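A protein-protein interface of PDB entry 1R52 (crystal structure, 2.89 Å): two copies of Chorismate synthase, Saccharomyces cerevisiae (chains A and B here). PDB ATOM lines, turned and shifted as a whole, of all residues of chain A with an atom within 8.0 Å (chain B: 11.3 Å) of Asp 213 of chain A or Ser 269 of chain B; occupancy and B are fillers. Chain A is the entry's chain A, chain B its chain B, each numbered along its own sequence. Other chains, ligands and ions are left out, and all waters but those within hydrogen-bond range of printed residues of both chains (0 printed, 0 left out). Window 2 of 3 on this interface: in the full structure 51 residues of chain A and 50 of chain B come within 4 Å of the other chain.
Among the printed residues, merely in contact across the chains: Val 313 of chain A with Asn 272 of chain B (3.2 Å), Val 313 of chain A with Gly 268 of chain B (3.2 Å), Ser 214 of chain A with Pro 267 of chain B (3.2 Å), Asp 213 of chain A with Pro 267 of chain B (3.5 Å), Ile 215 of chain A with Val 264 of chain B (3.5 Å), Ile 215 of chain A with Ser 265 of chain B (3.6 Å), Tyr 208 of chain A with Pro 267 of chain B (3.6 Å), Ser 312 of chain A with Gly 268 of chain B (3.7 Å), Ile 215 of chain A with Val 266 of chain B (3.8 Å) and Ile 215 of chain A with Pro 267 of chain B (3.8 Å).
No position is printed for both chains.
The side-chain carboxylate of Asp 213 of chain A sits at hydrogen-bond distance from the backbone NH of Gly 268 of chain B, at 3.3 Å.
The side-chain carboxylate (OD2) of Asp 213 of chain A sits at hydrogen-bond distance from the side-chain hydroxyl (OG) of Ser 269 of chain B (2.5 Å).
The backbone carbonyl oxygen (O) of Ser 214 of chain A sits at hydrogen-bond distance from the backbone NH (N) of Gly 268 of chain B (2.5 Å).
Printed residues of chain A that touch a printed residue of chain B: Tyr 208, Asp 213, Ser 214, Ile 215, Ser 312 and Val 313.
Hydrophobic or aromatic side chains of chain A within 4 Å of the printed part of chain B: Tyr 208, Ile 215 and Val 313.
Printed residues of chain B that touch a printed residue of chain A: Val 264, Ser 265, Val 266, Pro 267, Gly 268, Ser 269 and Asn 272.
Hydrophobic or aromatic side chains of chain B that line the printed part of chain A: Pro 267.
The backbone carbonyl oxygen (O) of Tyr 208 of chain A lies within hydrogen-bond range of the backbone NH (N) of Asp 213 of chain A, 2.9 Å away.
OG of Ser 214 of chain A sits at hydrogen-bond distance from ND1 of His 338 of chain A, 3.0 Å away.
The backbone carbonyl oxygen (O) of Pro 267 of chain B sits at hydrogen-bond distance from a ring nitrogen (ND1) of His 271 of chain B, 3.4 Å away.
The backbone carbonyl oxygen of Gly 268 of chain B lies within hydrogen-bond range of the side-chain amide nitrogen of Asn 272 of chain B (3.3 Å).
Of the printed residues of chain B, Asp 213 of chain A touches Pro 267 (3.5 Å), Gly 268 (3.3 Å) and Ser 269 (2.5 Å).
Of chain A, only Asp 213 comes within 4 Å of Ser 269 of chain B.
No residue of chain B comes within 4 Å of Gly 210 of chain A.
Asn 211 of chain A touches none of the printed residues of chain B.
Of chain B, only Pro 267 (3.2 Å) and Gly 268 (2.5 Å) come within 4 Å of Ser 214 of chain A.
No residue of chain B comes within 4 Å of His 338 of chain A.
Of the printed residues of chain B, Ser 312 of chain A touches Gly 268.
Of the printed residues of chain A, Ser 265 of chain B touches Ile 215.
Printed residues of chain B within 4 Å of Ile 215 of chain A: Val 264, Ser 265, Val 266 and Pro 267.
Of the printed residues of chain A, Val 264 of chain B touches Ile 215 (3.5 Å).
The nearest residue of chain A that does not touch Ser 269 of chain B is His 338 of chain A (4.1 Å).
The nearest printed residue of chain A that does not touch Val 264 of chain B is Ser 312 of chain A (5.7 Å).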
ATOM      1  N   ILE A 205      -6.454  16.618   9.678  1.00  0.00           N
ATOM      2  CA  ILE A 205      -6.191  17.448  10.859  1.00  0.00           C
ATOM      3  C   ILE A 205      -7.466  18.082  11.410  1.00  0.00           C
ATOM      4  O   ILE A 205      -7.603  18.287  12.621  1.00  0.00           O
ATOM      5  CB  ILE A 205      -5.078  18.511  10.619  1.00  0.00           C
ATOM      6  CG1 ILE A 205      -3.713  17.819  10.658  1.00  0.00           C
ATOM      7  CG2 ILE A 205      -5.101  19.589  11.699  1.00  0.00           C
ATOM      8  CD1 ILE A 205      -2.506  18.691  10.245  1.00  0.00           C
ATOM      9  N   GLU A 206      -8.387  18.384  10.510  1.00  0.00           N
ATOM     10  CA  GLU A 206      -9.664  19.020  10.838  1.00  0.00           C
ATOM     11  C   GLU A 206     -10.706  18.012  11.405  1.00  0.00           C
ATOM     12  O   GLU A 206     -11.415  18.301  12.369  1.00  0.00           O
ATOM     13  CB  GLU A 206     -10.199  19.774   9.600  1.00  0.00           C
ATOM     14  CG  GLU A 206      -9.516  21.132   9.388  1.00  0.00           C
ATOM     15  CD  GLU A 206      -9.548  22.015  10.640  1.00  0.00           C
ATOM     16  OE1 GLU A 206     -10.617  21.996  11.316  1.00  0.00           O
ATOM     17  OE2 GLU A 206      -8.521  22.698  10.967  1.00  0.00           O
ATOM     18  N   LYS A 207     -10.795  16.835  10.817  1.00  0.00           N
ATOM     19  CA  LYS A 207     -11.582  15.794  11.409  1.00  0.00           C
ATOM     20  C   LYS A 207     -11.370  15.761  12.918  1.00  0.00           C
ATOM     21  O   LYS A 207     -12.327  15.960  13.680  1.00  0.00           O
ATOM     22  CB  LYS A 207     -11.171  14.455  10.797  1.00  0.00           C
ATOM     23  CG  LYS A 207     -11.910  13.234  11.369  1.00  0.00           C
ATOM     24  CD  LYS A 207     -11.777  12.020  10.467  1.00  0.00           C
ATOM     25  CE  LYS A 207     -10.610  11.201  10.876  1.00  0.00           C
ATOM     26  NZ  LYS A 207     -10.798   9.843  10.387  1.00  0.00           N
ATOM     27  N   TYR A 208     -10.111  15.524  13.326  1.00  0.00           N
ATOM     28  CA  TYR A 208      -9.728  15.323  14.718  1.00  0.00           C
ATOM     29  C   TYR A 208      -9.807  16.600  15.496  1.00  0.00           C
ATOM     30  O   TYR A 208      -9.961  16.565  16.679  1.00  0.00           O
ATOM     31  CB  TYR A 208      -8.330  14.691  14.817  1.00  0.00           C
ATOM     32  CG  TYR A 208      -8.345  13.253  14.421  1.00  0.00           C
ATOM     33  CD1 TYR A 208      -9.025  12.343  15.181  1.00  0.00           C
ATOM     34  CD2 TYR A 208      -7.706  12.806  13.290  1.00  0.00           C
ATOM     35  CE1 TYR A 208      -9.071  11.035  14.867  1.00  0.00           C
ATOM     36  CE2 TYR A 208      -7.754  11.463  12.927  1.00  0.00           C
ATOM     37  CZ  TYR A 208      -8.463  10.587  13.746  1.00  0.00           C
ATOM     38  OH  TYR A 208      -8.588   9.256  13.472  1.00  0.00           O
ATOM     39  N   ARG A 209      -9.700  17.734  14.841  1.00  0.00           N
ATOM     40  CA  ARG A 209      -9.927  19.016  15.523  1.00  0.00           C
ATOM     41  C   ARG A 209     -11.387  19.162  15.917  1.00  0.00           C
ATOM     42  O   ARG A 209     -11.701  19.781  16.915  1.00  0.00           O
ATOM     43  CB  ARG A 209      -9.550  20.192  14.628  1.00  0.00           C
ATOM     44  CG  ARG A 209      -9.926  21.573  15.204  1.00  0.00           C
ATOM     45  CD  ARG A 209      -9.114  22.813  14.630  1.00  0.00           C
ATOM     46  NE  ARG A 209      -7.644  22.601  14.602  1.00  0.00           N
ATOM     47  CZ  ARG A 209      -6.722  23.480  14.131  1.00  0.00           C
ATOM     48  NH1 ARG A 209      -7.079  24.689  13.664  1.00  0.00           N
ATOM     49  NH2 ARG A 209      -5.417  23.143  14.156  1.00  0.00           N
ATOM     50  N   GLY A 210     -12.256  18.586  15.102  1.00  0.00           N
ATOM     51  CA  GLY A 210     -13.663  18.596  15.329  1.00  0.00           C
ATOM     52  C   GLY A 210     -14.067  17.822  16.559  1.00  0.00           C
ATOM     53  O   GLY A 210     -14.852  18.320  17.355  1.00  0.00           O
ATOM     54  N   ASN A 211     -13.522  16.618  16.727  1.00  0.00           N
ATOM     55  CA  ASN A 211     -13.768  15.779  17.911  1.00  0.00           C
ATOM     56  C   ASN A 211     -12.962  16.177  19.185  1.00  0.00           C
ATOM     57  O   ASN A 211     -13.024  15.495  20.197  1.00  0.00           O
ATOM     58  CB  ASN A 211     -13.491  14.338  17.528  1.00  0.00           C
ATOM     59  CG  ASN A 211     -14.031  14.006  16.125  1.00  0.00           C
ATOM     60  OD1 ASN A 211     -15.223  14.323  15.814  1.00  0.00           O
ATOM     61  ND2 ASN A 211     -13.179  13.380  15.260  1.00  0.00           N
ATOM     62  N   LYS A 212     -12.259  17.316  19.123  1.00  0.00           N
ATOM     63  CA  LYS A 212     -11.457  17.847  20.213  1.00  0.00           C
ATOM     64  C   LYS A 212     -10.405  16.813  20.576  1.00  0.00           C
ATOM     65  O   LYS A 212     -10.097  16.583  21.741  1.00  0.00           O
ATOM     66  CB  LYS A 212     -12.358  18.190  21.411  1.00  0.00           C
ATOM     67  CG  LYS A 212     -13.528  19.107  21.089  1.00  0.00           C
ATOM     68  CD  LYS A 212     -14.196  19.610  22.386  1.00  0.00           C
ATOM     69  CE  LYS A 212     -15.592  20.312  22.154  1.00  0.00           C
ATOM     70  NZ  LYS A 212     -16.667  19.356  21.542  1.00  0.00           N
ATOM     71  N   ASP A 213      -9.913  16.159  19.529  1.00  0.00           N
ATOM     72  CA  ASP A 213      -8.885  15.101  19.588  1.00  0.00           C
ATOM     73  C   ASP A 213      -7.582  15.593  18.952  1.00  0.00           C
ATOM     74  O   ASP A 213      -7.371  16.810  18.791  1.00  0.00           O
ATOM     75  CB  ASP A 213      -9.376  13.831  18.860  1.00  0.00           C
ATOM     76  CG  ASP A 213      -8.795  12.540  19.462  1.00  0.00           C
ATOM     77  OD1 ASP A 213      -7.710  12.619  20.036  1.00  0.00           O
ATOM     78  OD2 ASP A 213      -9.324  11.412  19.429  1.00  0.00           O
ATOM     79  N   SER A 214      -6.716  14.657  18.592  1.00  0.00           N
ATOM     80  CA  SER A 214      -5.440  14.967  17.949  1.00  0.00           C
ATOM     81  C   SER A 214      -4.855  13.729  17.395  1.00  0.00           C
ATOM     82  O   SER A 214      -5.283  12.591  17.724  1.00  0.00           O
ATOM     83  CB  SER A 214      -4.402  15.468  18.922  1.00  0.00           C
ATOM     84  OG  SER A 214      -4.086  14.408  19.820  1.00  0.00           O
ATOM     85  N   ILE A 215      -3.837  13.958  16.572  1.00  0.00           N
ATOM     86  CA  ILE A 215      -3.238  12.895  15.774  1.00  0.00           C
ATOM     87  C   ILE A 215      -1.819  13.309  15.415  1.00  0.00           C
ATOM     88  O   ILE A 215      -1.518  14.475  15.083  1.00  0.00           O
ATOM     89  CB  ILE A 215      -4.077  12.635  14.582  1.00  0.00           C
ATOM     90  CG1 ILE A 215      -3.605  11.426  13.849  1.00  0.00           C
ATOM     91  CG2 ILE A 215      -3.994  13.810  13.679  1.00  0.00           C
ATOM     92  CD1 ILE A 215      -4.406  10.230  14.089  1.00  0.00           C
ATOM     93  N   SER A 312       0.930  12.715  18.953  1.00  0.00           N
ATOM     94  CA  SER A 312      -0.137  13.752  19.066  1.00  0.00           C
ATOM     95  C   SER A 312      -0.261  14.556  20.399  1.00  0.00           C
ATOM     96  O   SER A 312      -0.652  15.731  20.416  1.00  0.00           O
ATOM     97  CB  SER A 312      -1.476  13.011  18.814  1.00  0.00           C
ATOM     98  OG  SER A 312      -1.380  11.531  18.788  1.00  0.00           O
ATOM     99  N   VAL A 313       0.070  13.887  21.499  1.00  0.00           N
ATOM    100  CA  VAL A 313      -0.273  14.295  22.862  1.00  0.00           C
ATOM    101  C   VAL A 313       0.846  14.194  23.884  1.00  0.00           C
ATOM    102  O   VAL A 313       0.797  13.330  24.802  1.00  0.00           O
ATOM    103  CB  VAL A 313      -1.469  13.337  23.426  1.00  0.00           C
ATOM    104  CG1 VAL A 313      -2.587  14.119  24.078  1.00  0.00           C
ATOM    105  CG2 VAL A 313      -1.974  12.348  22.364  1.00  0.00           C
ATOM    106  N   ARG A 337      -2.516  18.419  27.132  1.00  0.00           N
ATOM    107  CA  ARG A 337      -2.886  19.131  25.908  1.00  0.00           C
ATOM    108  C   ARG A 337      -2.694  18.210  24.672  1.00  0.00           C
ATOM    109  O   ARG A 337      -2.083  17.124  24.766  1.00  0.00           O
ATOM    110  CB  ARG A 337      -2.106  20.470  25.763  1.00  0.00           C
ATOM    111  N   HIS A 338      -3.227  18.670  23.534  1.00  0.00           N
ATOM    112  CA  HIS A 338      -3.269  17.924  22.284  1.00  0.00           C
ATOM    113  C   HIS A 338      -2.316  18.619  21.269  1.00  0.00           C
ATOM    114  O   HIS A 338      -1.128  18.800  21.537  1.00  0.00           O
ATOM    115  CB  HIS A 338      -4.759  17.840  21.790  1.00  0.00           C
ATOM    116  CG  HIS A 338      -5.568  16.698  22.372  1.00  0.00           C
ATOM    117  ND1 HIS A 338      -5.120  15.391  22.414  1.00  0.00           N
ATOM    118  CD2 HIS A 338      -6.814  16.668  22.904  1.00  0.00           C
ATOM    119  CE1 HIS A 338      -6.038  14.616  22.975  1.00  0.00           C
ATOM    120  NE2 HIS A 338      -7.077  15.366  23.283  1.00  0.00           N
ATOM    121  N   ASP A 339      -2.859  18.958  20.095  1.00  0.00           N
ATOM    122  CA  ASP A 339      -2.279  19.868  19.087  1.00  0.00           C
ATOM    123  C   ASP A 339      -3.421  20.297  18.064  1.00  0.00           C
ATOM    124  O   ASP A 339      -3.942  21.412  18.187  1.00  0.00           O
ATOM    125  CB  ASP A 339      -0.964  19.326  18.479  1.00  0.00           C
ATOM    126  CG  ASP A 339       0.228  20.300  18.689  1.00  0.00           C
ATOM    127  OD1 ASP A 339       0.233  21.418  18.123  1.00  0.00           O
ATOM    128  OD2 ASP A 339       1.219  20.033  19.396  1.00  0.00           O
ATOM    129  N   PRO A 340      -3.833  19.501  17.072  1.00  0.00           N
ATOM    130  CA  PRO A 340      -3.112  18.338  16.487  1.00  0.00           C
ATOM    131  C   PRO A 340      -2.054  18.695  15.412  1.00  0.00           C
ATOM    132  O   PRO A 340      -1.558  17.834  14.691  1.00  0.00           O
ATOM    133  CB  PRO A 340      -4.230  17.536  15.821  1.00  0.00           C
ATOM    134  CG  PRO A 340      -5.407  18.573  15.569  1.00  0.00           C
ATOM    135  CD  PRO A 340      -5.150  19.757  16.455  1.00  0.00           C
ATOM    136  N   ALA A 341      -1.713  19.978  15.352  1.00  0.00           N
ATOM    137  CA  ALA A 341      -0.707  20.539  14.466  1.00  0.00           C
ATOM    138  C   ALA A 341       0.755  20.309  14.939  1.00  0.00           C
ATOM    139  O   ALA A 341       1.642  21.169  14.692  1.00  0.00           O
ATOM    140  CB  ALA A 341      -0.948  22.085  14.355  1.00  0.00           C
ATOM    141  N   SER B 167       1.032  -1.851  19.696  1.00  0.00           N
ATOM    142  CA  SER B 167       1.153  -1.516  21.109  1.00  0.00           C
ATOM    143  C   SER B 167      -0.235  -1.593  21.768  1.00  0.00           C
ATOM    144  O   SER B 167      -0.363  -1.751  22.973  1.00  0.00           O
ATOM    145  CB  SER B 167       1.801  -0.168  21.279  1.00  0.00           C
ATOM    146  OG  SER B 167       0.844   0.863  21.090  1.00  0.00           O
ATOM    147  N   PHE B 168      -1.283  -1.529  20.957  1.00  0.00           N
ATOM    148  CA  PHE B 168      -2.637  -1.557  21.490  1.00  0.00           C
ATOM    149  C   PHE B 168      -3.215  -2.948  21.603  1.00  0.00           C
ATOM    150  O   PHE B 168      -4.248  -3.131  22.245  1.00  0.00           O
ATOM    151  CB  PHE B 168      -3.552  -0.691  20.675  1.00  0.00           C
ATOM    152  CG  PHE B 168      -3.144   0.759  20.641  1.00  0.00           C
ATOM    153  CD1 PHE B 168      -3.861   1.707  21.358  1.00  0.00           C
ATOM    154  CD2 PHE B 168      -2.066   1.197  19.842  1.00  0.00           C
ATOM    155  CE1 PHE B 168      -3.509   3.089  21.303  1.00  0.00           C
ATOM    156  CE2 PHE B 168      -1.715   2.568  19.792  1.00  0.00           C
ATOM    157  CZ  PHE B 168      -2.467   3.507  20.551  1.00  0.00           C
ATOM    158  N   SER B 259       4.741   3.313  20.826  1.00  0.00           N
ATOM    159  CA  SER B 259       3.787   3.288  19.717  1.00  0.00           C
ATOM    160  C   SER B 259       4.504   3.492  18.414  1.00  0.00           C
ATOM    161  O   SER B 259       4.060   3.042  17.366  1.00  0.00           O
ATOM    162  CB  SER B 259       2.662   4.321  19.914  1.00  0.00           C
ATOM    163  OG  SER B 259       3.143   5.672  20.164  1.00  0.00           O
ATOM    164  N   GLY B 263       1.801   3.978  15.611  1.00  0.00           N
ATOM    165  CA  GLY B 263       0.831   4.761  16.356  1.00  0.00           C
ATOM    166  C   GLY B 263       0.558   6.179  15.854  1.00  0.00           C
ATOM    167  O   GLY B 263      -0.166   6.946  16.466  1.00  0.00           O
ATOM    168  N   VAL B 264       1.194   6.560  14.765  1.00  0.00           N
ATOM    169  CA  VAL B 264       1.020   7.868  14.217  1.00  0.00           C
ATOM    170  C   VAL B 264      -0.377   7.942  13.628  1.00  0.00           C
ATOM    171  O   VAL B 264      -1.039   8.992  13.657  1.00  0.00           O
ATOM    172  CB  VAL B 264       2.029   8.088  13.117  1.00  0.00           C
ATOM    173  CG1 VAL B 264       1.793   9.416  12.444  1.00  0.00           C
ATOM    174  CG2 VAL B 264       3.449   8.057  13.664  1.00  0.00           C
ATOM    175  N   SER B 265      -0.834   6.811  13.103  1.00  0.00           N
ATOM    176  CA  SER B 265      -2.182   6.741  12.578  1.00  0.00           C
ATOM    177  C   SER B 265      -3.307   6.601  13.611  1.00  0.00           C
ATOM    178  O   SER B 265      -4.460   6.754  13.265  1.00  0.00           O
ATOM    179  CB  SER B 265      -2.273   5.601  11.613  1.00  0.00           C
ATOM    180  OG  SER B 265      -2.334   4.471  12.437  1.00  0.00           O
ATOM    181  N   VAL B 266      -2.986   6.333  14.854  1.00  0.00           N
ATOM    182  CA  VAL B 266      -3.967   6.282  15.958  1.00  0.00           C
ATOM    183  C   VAL B 266      -4.050   7.599  16.743  1.00  0.00           C
ATOM    184  O   VAL B 266      -3.024   8.164  17.078  1.00  0.00           O
ATOM    185  CB  VAL B 266      -3.577   5.217  16.971  1.00  0.00           C
ATOM    186  CG1 VAL B 266      -4.484   5.277  18.195  1.00  0.00           C
ATOM    187  CG2 VAL B 266      -3.548   3.838  16.322  1.00  0.00           C
ATOM    188  N   PRO B 267      -5.272   8.059  17.038  1.00  0.00           N
ATOM    189  CA  PRO B 267      -5.524   9.367  17.664  1.00  0.00           C
ATOM    190  C   PRO B 267      -5.074   9.546  19.097  1.00  0.00           C
ATOM    191  O   PRO B 267      -4.877   8.620  19.880  1.00  0.00           O
ATOM    192  CB  PRO B 267      -7.048   9.464  17.655  1.00  0.00           C
ATOM    193  CG  PRO B 267      -7.536   8.383  16.779  1.00  0.00           C
ATOM    194  CD  PRO B 267      -6.531   7.350  16.761  1.00  0.00           C
ATOM    195  N   GLY B 268      -4.976  10.794  19.461  1.00  0.00           N
ATOM    196  CA  GLY B 268      -4.488  11.121  20.769  1.00  0.00           C
ATOM    197  C   GLY B 268      -5.272  10.416  21.864  1.00  0.00           C
ATOM    198  O   GLY B 268      -4.754   9.680  22.707  1.00  0.00           O
ATOM    199  N   SER B 269      -6.565  10.668  21.863  1.00  0.00           N
ATOM    200  CA  SER B 269      -7.451  10.036  22.829  1.00  0.00           C
ATOM    201  C   SER B 269      -7.129   8.527  23.017  1.00  0.00           C
ATOM    202  O   SER B 269      -6.924   8.114  24.153  1.00  0.00           O
ATOM    203  CB  SER B 269      -8.924  10.293  22.470  1.00  0.00           C
ATOM    204  OG  SER B 269      -9.316   9.697  21.252  1.00  0.00           O
ATOM    205  N   LYS B 270      -7.012   7.750  21.930  1.00  0.00           N
ATOM    206  CA  LYS B 270      -6.809   6.306  22.064  1.00  0.00           C
ATOM    207  C   LYS B 270      -5.461   5.918  22.707  1.00  0.00           C
ATOM    208  O   LYS B 270      -5.305   4.852  23.328  1.00  0.00           O
ATOM    209  CB  LYS B 270      -7.076   5.588  20.748  1.00  0.00           C
ATOM    210  CG  LYS B 270      -8.558   5.182  20.644  1.00  0.00           C
ATOM    211  CD  LYS B 270      -9.044   4.981  19.172  1.00  0.00           C
ATOM    212  CE  LYS B 270     -10.427   4.294  19.037  1.00  0.00           C
ATOM    213  NZ  LYS B 270     -10.467   2.950  19.735  1.00  0.00           N
ATOM    214  N   HIS B 271      -4.498   6.822  22.593  1.00  0.00           N
ATOM    215  CA  HIS B 271      -3.187   6.652  23.221  1.00  0.00           C
ATOM    216  C   HIS B 271      -3.275   6.737  24.740  1.00  0.00           C
ATOM    217  O   HIS B 271      -2.754   5.868  25.436  1.00  0.00           O
ATOM    218  CB  HIS B 271      -2.241   7.738  22.729  1.00  0.00           C
ATOM    219  CG  HIS B 271      -1.401   7.318  21.571  1.00  0.00           C
ATOM    220  ND1 HIS B 271      -1.936   6.954  20.362  1.00  0.00           N
ATOM    221  CD2 HIS B 271      -0.061   7.217  21.432  1.00  0.00           C
ATOM    222  CE1 HIS B 271      -0.968   6.620  19.534  1.00  0.00           C
ATOM    223  NE2 HIS B 271       0.180   6.781  20.158  1.00  0.00           N
ATOM    224  N   ASN B 272      -3.933   7.782  25.245  1.00  0.00           N
ATOM    225  CA  ASN B 272      -3.913   8.116  26.680  1.00  0.00           C
ATOM    226  C   ASN B 272      -5.108   7.716  27.490  1.00  0.00           C
ATOM    227  O   ASN B 272      -5.096   7.896  28.690  1.00  0.00           O
ATOM    228  CB  ASN B 272      -3.732   9.620  26.888  1.00  0.00           C
ATOM    229  CG  ASN B 272      -2.690  10.176  25.992  1.00  0.00           C
ATOM    230  OD1 ASN B 272      -1.552   9.722  26.014  1.00  0.00           O
ATOM    231  ND2 ASN B 272      -3.070  11.133  25.152  1.00  0.00           N
ATOM    232  N   ASP B 273      -6.138   7.195  26.855  1.00  0.00           N
ATOM    233  CA  ASP B 273      -7.367   6.857  27.567  1.00  0.00           C
ATOM    234  C   ASP B 273      -7.073   5.643  28.434  1.00  0.00           C
ATOM    235  O   ASP B 273      -6.401   4.732  27.941  1.00  0.00           O
ATOM    236  CB  ASP B 273      -8.516   6.522  26.577  1.00  0.00           C
ATOM    237  CG  ASP B 273      -9.478   7.717  26.312  1.00  0.00           C
ATOM    238  OD1 ASP B 273      -9.133   8.904  26.584  1.00  0.00           O
ATOM    239  OD2 ASP B 273     -10.608   7.541  25.795  1.00  0.00           O
ATOM    240  N   PRO B 274      -7.595   5.616  29.679  1.00  0.00           N
ATOM    241  CA  PRO B 274      -7.492   4.442  30.587  1.00  0.00           C
ATOM    242  C   PRO B 274      -8.266   3.188  30.158  1.00  0.00           C
ATOM    243  O   PRO B 274      -7.986   2.118  30.691  1.00  0.00           O
ATOM    244  CB  PRO B 274      -8.103   4.926  31.917  1.00  0.00           C
ATOM    245  CG  PRO B 274      -8.387   6.424  31.767  1.00  0.00           C
ATOM    246  CD  PRO B 274      -8.368   6.720  30.289  1.00  0.00           C
ATOM    247  N   PHE B 275      -9.239   3.334  29.252  1.00  0.00           N
ATOM    248  CA  PHE B 275      -9.935   2.207  28.612  1.00  0.00           C
ATOM    249  C   PHE B 275      -9.931   2.456  27.119  1.00  0.00           C
ATOM    250  O   PHE B 275     -10.266   3.571  26.708  1.00  0.00           O
ATOM    251  CB  PHE B 275     -11.366   2.136  29.126  1.00  0.00           C
ATOM    252  CG  PHE B 275     -11.467   2.118  30.644  1.00  0.00           C
ATOM    253  CD1 PHE B 275     -11.478   0.911  31.336  1.00  0.00           C
ATOM    254  CD2 PHE B 275     -11.541   3.302  31.379  1.00  0.00           C
ATOM    255  CE1 PHE B 275     -11.568   0.894  32.723  1.00  0.00           C
ATOM    256  CE2 PHE B 275     -11.617   3.281  32.773  1.00  0.00           C
ATOM    257  CZ  PHE B 275     -11.630   2.081  33.434  1.00  0.00           C
ATOM    258  N   TYR B 276      -9.518   1.458  26.314  1.00  0.00           N
ATOM    259  CA  TYR B 276      -9.558   1.545  24.804  1.00  0.00           C
ATOM    260  C   TYR B 276     -10.347   0.383  24.166  1.00  0.00           C
ATOM    261  O   TYR B 276     -10.610  -0.620  24.814  1.00  0.00           O
ATOM    262  CB  TYR B 276      -8.155   1.676  24.154  1.00  0.00           C
ATOM    263  N   THR B 286      -8.195  -1.674  30.062  1.00  0.00           N
ATOM    264  CA  THR B 286      -7.215  -0.899  30.810  1.00  0.00           C
ATOM    265  C   THR B 286      -5.999  -0.539  29.915  1.00  0.00           C
ATOM    266  O   THR B 286      -5.209  -1.417  29.489  1.00  0.00           O
ATOM    267  CB  THR B 286      -6.798  -1.627  32.130  1.00  0.00           C
ATOM    268  N   LYS B 287      -5.877   0.766  29.634  1.00  0.00           N
ATOM    269  CA  LYS B 287      -4.743   1.333  28.874  1.00  0.00           C
ATOM    270  C   LYS B 287      -3.430   0.493  28.969  1.00  0.00           C
ATOM    271  O   LYS B 287      -3.013   0.043  30.049  1.00  0.00           O
ATOM    272  CB  LYS B 287      -4.482   2.811  29.284  1.00  0.00           C
ATOM    273  N   THR B 288      -2.804   0.313  27.806  1.00  0.00           N
ATOM    274  CA  THR B 288      -1.525  -0.395  27.687  1.00  0.00           C
ATOM    275  C   THR B 288      -0.313   0.542  27.569  1.00  0.00           C
ATOM    276  O   THR B 288      -0.421   1.720  27.297  1.00  0.00           O
ATOM    277  CB  THR B 288      -1.549  -1.352  26.484  1.00  0.00           C
ATOM    278  OG1 THR B 288      -1.966  -0.649  25.295  1.00  0.00           O
ATOM    279  CG2 THR B 288      -2.560  -2.499  26.716  1.00  0.00           C
ATOM    280  N   ASN B 290       1.934   2.452  25.830  1.00  0.00           N
ATOM    281  CA  ASN B 290       2.062   3.088  24.525  1.00  0.00           C
ATOM    282  C   ASN B 290       3.303   4.012  24.444  1.00  0.00           C
ATOM    283  O   ASN B 290       3.847   4.264  23.365  1.00  0.00           O
ATOM    284  CB  ASN B 290       0.760   3.852  24.195  1.00  0.00           C
ATOM    285  CG  ASN B 290      -0.442   2.894  23.954  1.00  0.00           C
ATOM    286  OD1 ASN B 290      -0.393   2.049  23.052  1.00  0.00           O
ATOM    287  ND2 ASN B 290      -1.498   3.012  24.762  1.00  0.00           N
